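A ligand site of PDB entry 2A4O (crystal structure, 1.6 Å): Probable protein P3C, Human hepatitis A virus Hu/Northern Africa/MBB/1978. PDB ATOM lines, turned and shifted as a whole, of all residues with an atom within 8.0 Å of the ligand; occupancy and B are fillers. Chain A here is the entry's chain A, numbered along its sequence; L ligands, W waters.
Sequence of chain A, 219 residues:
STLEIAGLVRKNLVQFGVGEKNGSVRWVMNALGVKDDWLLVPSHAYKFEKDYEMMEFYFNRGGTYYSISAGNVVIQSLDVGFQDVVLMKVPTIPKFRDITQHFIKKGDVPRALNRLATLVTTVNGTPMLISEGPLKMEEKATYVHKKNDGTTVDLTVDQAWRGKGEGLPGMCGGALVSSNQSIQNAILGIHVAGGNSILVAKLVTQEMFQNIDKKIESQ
A carbon (C3) of the ligand is bonded to a ring nitrogen (NE2) of His 102 (1.4 Å).
NH2 of Arg 97 lies close to O1 of the ligand (2.7 Å).
The side-chain hydroxyl of Thr 100 lies within hydrogen-bond range of the side-chain amide oxygen of Gln 101 (2.9 Å).
The backbone carbonyl oxygen (O) of Gln 101 sits close to the side-chain amide oxygen (OE1) of Gln 206, 3.2 Å away.
The backbone NH (N) of Ile 187 sits at hydrogen-bond distance from the backbone carbonyl oxygen (O) of His 102, 2.8 Å away.
Residues that only touch the ligand: Leu 8 (3.4 Å) and Gln 101 (3.6 Å).
Water W3 lies within hydrogen-bond range of the backbone carbonyl oxygen of Asp 98 (2.6 Å) and the guanidinium group of Arg 97 (2.8 Å).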
ATOM      1  N   GLU A   4       3.405 -14.922 -12.236  1.00  0.00           N
ATOM      2  CA  GLU A   4       2.731 -13.974 -13.126  1.00  0.00           C
ATOM      3  C   GLU A   4       2.180 -12.746 -12.397  1.00  0.00           C
ATOM      4  O   GLU A   4       2.296 -11.618 -12.906  1.00  0.00           O
ATOM      5  CB  GLU A   4       1.658 -14.652 -13.987  1.00  0.00           C
ATOM      6  CG  GLU A   4       2.239 -15.706 -14.938  1.00  0.00           C
ATOM      7  CD  GLU A   4       3.103 -15.130 -16.060  1.00  0.00           C
ATOM      8  OE1 GLU A   4       2.916 -13.950 -16.450  1.00  0.00           O
ATOM      9  OE2 GLU A   4       3.966 -15.886 -16.568  1.00  0.00           O
ATOM     10  N   ILE A   5       1.568 -12.947 -11.232  1.00  0.00           N
ATOM     11  CA  ILE A   5       1.200 -11.799 -10.378  1.00  0.00           C
ATOM     12  C   ILE A   5       2.428 -10.964 -10.069  1.00  0.00           C
ATOM     13  O   ILE A   5       2.385  -9.729 -10.163  1.00  0.00           O
ATOM     14  CB  ILE A   5       0.551 -12.203  -9.041  1.00  0.00           C
ATOM     15  CG1 ILE A   5      -0.818 -12.813  -9.297  1.00  0.00           C
ATOM     16  CG2 ILE A   5       0.463 -10.969  -8.058  1.00  0.00           C
ATOM     17  CD1 ILE A   5      -1.870 -11.830  -9.856  1.00  0.00           C
ATOM     18  N   LEU A   8       3.314  -8.598 -12.810  1.00  0.00           N
ATOM     19  CA  LEU A   8       2.434  -7.416 -12.825  1.00  0.00           C
ATOM     20  C   LEU A   8       2.817  -6.413 -11.744  1.00  0.00           C
ATOM     21  O   LEU A   8       2.806  -5.195 -11.973  1.00  0.00           O
ATOM     22  CB  LEU A   8       0.964  -7.813 -12.677  1.00  0.00           C
ATOM     23  CG  LEU A   8       0.372  -8.721 -13.768  1.00  0.00           C
ATOM     24  CD1 LEU A   8      -1.028  -9.059 -13.362  1.00  0.00           C
ATOM     25  CD2 LEU A   8       0.397  -8.040 -15.111  1.00  0.00           C
ATOM     26  N   ARG A  97      -1.025   0.500 -15.378  1.00  0.00           N
ATOM     27  CA  ARG A  97      -1.947  -0.614 -15.558  1.00  0.00           C
ATOM     28  C   ARG A  97      -2.733  -0.807 -14.270  1.00  0.00           C
ATOM     29  O   ARG A  97      -2.138  -0.808 -13.187  1.00  0.00           O
ATOM     30  CB  ARG A  97      -1.179  -1.891 -15.867  1.00  0.00           C
ATOM     31  CG  ARG A  97      -2.040  -3.113 -16.009  1.00  0.00           C
ATOM     32  CD  ARG A  97      -1.161  -4.314 -16.312  1.00  0.00           C
ATOM     33  NE  ARG A  97      -1.957  -5.490 -16.600  1.00  0.00           N
ATOM     34  CZ  ARG A  97      -1.549  -6.514 -17.347  1.00  0.00           C
ATOM     35  NH1 ARG A  97      -0.344  -6.481 -17.916  1.00  0.00           N
ATOM     36  NH2 ARG A  97      -2.353  -7.555 -17.550  1.00  0.00           N
ATOM     37  N   ASP A  98      -4.044  -0.930 -14.388  1.00  0.00           N
ATOM     38  CA  ASP A  98      -4.936  -1.127 -13.227  1.00  0.00           C
ATOM     39  C   ASP A  98      -4.741  -2.548 -12.691  1.00  0.00           C
ATOM     40  O   ASP A  98      -5.100  -3.527 -13.377  1.00  0.00           O
ATOM     41  CB  ASP A  98      -6.402  -0.899 -13.654  1.00  0.00           C
ATOM     42  CG  ASP A  98      -7.386  -1.027 -12.504  1.00  0.00           C
ATOM     43  OD1 ASP A  98      -6.967  -1.358 -11.369  1.00  0.00           O
ATOM     44  OD2 ASP A  98      -8.601  -0.792 -12.758  1.00  0.00           O
ATOM     45  N   ILE A  99      -4.144  -2.644 -11.503  1.00  0.00           N
ATOM     46  CA  ILE A  99      -3.961  -3.957 -10.848  1.00  0.00           C
ATOM     47  C   ILE A  99      -4.858  -4.110  -9.602  1.00  0.00           C
ATOM     48  O   ILE A  99      -4.718  -5.052  -8.828  1.00  0.00           O
ATOM     49  CB  ILE A  99      -2.485  -4.267 -10.502  1.00  0.00           C
ATOM     50  CG1 ILE A  99      -1.878  -3.183  -9.606  1.00  0.00           C
ATOM     51  CG2 ILE A  99      -1.647  -4.421 -11.776  1.00  0.00           C
ATOM     52  CD1 ILE A  99      -0.528  -3.569  -9.052  1.00  0.00           C
ATOM     53  N   THR A 100      -5.783  -3.168  -9.421  1.00  0.00           N
ATOM     54  CA  THR A 100      -6.673  -3.208  -8.239  1.00  0.00           C
ATOM     55  C   THR A 100      -7.435  -4.526  -8.097  1.00  0.00           C
ATOM     56  O   THR A 100      -7.645  -4.980  -6.981  1.00  0.00           O
ATOM     57  CB  THR A 100      -7.664  -2.018  -8.179  1.00  0.00           C
ATOM     58  OG1 THR A 100      -8.514  -2.010  -9.333  1.00  0.00           O
ATOM     59  CG2 THR A 100      -6.886  -0.697  -8.059  1.00  0.00           C
ATOM     60  N   GLN A 101      -7.844  -5.120  -9.216  1.00  0.00           N
ATOM     61  CA  GLN A 101      -8.640  -6.365  -9.163  1.00  0.00           C
ATOM     62  C   GLN A 101      -7.830  -7.601  -8.785  1.00  0.00           C
ATOM     63  O   GLN A 101      -8.395  -8.690  -8.573  1.00  0.00           O
ATOM     64  CB  GLN A 101      -9.416  -6.564 -10.460  1.00  0.00           C
ATOM     65  CG  GLN A 101     -10.281  -5.350 -10.807  1.00  0.00           C
ATOM     66  CD  GLN A 101     -11.085  -4.847  -9.612  1.00  0.00           C
ATOM     67  OE1 GLN A 101     -10.806  -3.777  -9.060  1.00  0.00           O
ATOM     68  NE2 GLN A 101     -12.063  -5.639  -9.193  1.00  0.00           N
ATOM     69  N   HIS A 102      -6.522  -7.440  -8.683  1.00  0.00           N
ATOM     70  CA  HIS A 102      -5.629  -8.512  -8.233  1.00  0.00           C
ATOM     71  C   HIS A 102      -5.437  -8.526  -6.716  1.00  0.00           C
ATOM     72  O   HIS A 102      -4.785  -9.422  -6.190  1.00  0.00           O
ATOM     73  CB  HIS A 102      -4.284  -8.444  -8.949  1.00  0.00           C
ATOM     74  CG  HIS A 102      -4.378  -8.806 -10.406  1.00  0.00           C
ATOM     75  ND1 HIS A 102      -4.717 -10.076 -10.822  1.00  0.00           N
ATOM     76  CD2 HIS A 102      -4.161  -8.076 -11.524  1.00  0.00           C
ATOM     77  CE1 HIS A 102      -4.707 -10.108 -12.141  1.00  0.00           C
ATOM     78  NE2 HIS A 102      -4.386  -8.905 -12.600  1.00  0.00           N
ATOM     79  N   GLN A 184      -6.417 -16.852  -6.794  1.00  0.00           N
ATOM     80  CA  GLN A 184      -5.615 -16.258  -7.881  1.00  0.00           C
ATOM     81  C   GLN A 184      -4.366 -15.527  -7.348  1.00  0.00           C
ATOM     82  O   GLN A 184      -3.990 -14.460  -7.870  1.00  0.00           O
ATOM     83  CB  GLN A 184      -6.489 -15.355  -8.771  1.00  0.00           C
ATOM     84  CG  GLN A 184      -7.614 -16.089  -9.492  1.00  0.00           C
ATOM     85  CD  GLN A 184      -8.744 -16.494  -8.559  1.00  0.00           C
ATOM     86  OE1 GLN A 184      -9.253 -15.686  -7.808  1.00  0.00           O
ATOM     87  NE2 GLN A 184      -9.121 -17.772  -8.600  1.00  0.00           N
ATOM     88  N   ILE A 187      -2.810 -10.281  -4.342  1.00  0.00           N
ATOM     89  CA  ILE A 187      -1.954  -9.347  -3.626  1.00  0.00           C
ATOM     90  C   ILE A 187      -2.646  -9.031  -2.287  1.00  0.00           C
ATOM     91  O   ILE A 187      -3.826  -8.686  -2.257  1.00  0.00           O
ATOM     92  CB  ILE A 187      -1.761  -8.051  -4.428  1.00  0.00           C
ATOM     93  CG1 ILE A 187      -1.121  -8.345  -5.782  1.00  0.00           C
ATOM     94  CG2 ILE A 187      -0.887  -7.063  -3.643  1.00  0.00           C
ATOM     95  CD1 ILE A 187      -1.264  -7.194  -6.790  1.00  0.00           C
ATOM     96  N   GLN A 206      -9.219  -5.081  -1.916  1.00  0.00           N
ATOM     97  CA  GLN A 206      -9.854  -4.508  -3.090  1.00  0.00           C
ATOM     98  C   GLN A 206     -10.819  -3.370  -2.727  1.00  0.00           C
ATOM     99  O   GLN A 206     -10.872  -2.337  -3.388  1.00  0.00           O
ATOM    100  CB  GLN A 206     -10.626  -5.602  -3.786  1.00  0.00           C
ATOM    101  CG  GLN A 206     -10.309  -5.733  -5.207  1.00  0.00           C
ATOM    102  CD  GLN A 206     -11.033  -6.895  -5.789  1.00  0.00           C
ATOM    103  OE1 GLN A 206     -10.424  -7.909  -6.180  1.00  0.00           O
ATOM    104  NE2 GLN A 206     -12.352  -6.794  -5.844  1.00  0.00           N
HETATM  105  O1  LIG L   1      -4.545  -6.666 -16.161  1.00  0.00           O
HETATM  106  C1  LIG L   1      -5.491  -7.449 -15.902  1.00  0.00           C
HETATM  107  O2  LIG L   1      -6.358  -7.786 -16.768  1.00  0.00           O
HETATM  108  C2  LIG L   1      -5.600  -7.966 -14.486  1.00  0.00           C
HETATM  109  C3  LIG L   1      -4.309  -8.605 -13.945  1.00  0.00           C
HETATM  110  N1  LIG L   1      -6.717  -8.870 -14.345  1.00  0.00           N
HETATM  111  C4  LIG L   1      -7.909  -8.408 -14.012  1.00  0.00           C
HETATM  112  O3  LIG L   1      -8.183  -7.228 -13.812  1.00  0.00           O
HETATM  113  O4  LIG L   1      -8.936  -9.406 -13.890  1.00  0.00           O
HETATM  114  C5  LIG L   1     -10.305  -9.030 -13.774  1.00  0.00           C
HETATM  115  C6  LIG L   1     -11.078 -10.210 -14.304  1.00  0.00           C
HETATM  116  C7  LIG L   1     -12.448 -10.307 -14.077  1.00  0.00           C
HETATM  117  C8  LIG L   1     -13.134 -11.411 -14.586  1.00  0.00           C
HETATM  118  C9  LIG L   1     -12.465 -12.391 -15.329  1.00  0.00           C
HETATM  119  C10 LIG L   1     -11.102 -12.289 -15.579  1.00  0.00           C
HETATM  120  C11 LIG L   1     -10.407 -11.191 -15.057  1.00  0.00           C
HETATM  121  O   HOH W   1      -7.075  -5.093 -12.081  1.00  0.00           O
HETATM  122  O   HOH W   2      -8.567 -10.454 -10.979  1.00  0.00           O
HETATM  123  O   HOH W   3      -3.558  -5.447 -14.250  1.00  0.00           O
HETATM  124  O   HOH W   4      -5.161  -6.531 -18.974  1.00  0.00           O
HETATM  125  O   HOH W   5      -5.674  -4.041 -16.139  1.00  0.00           O
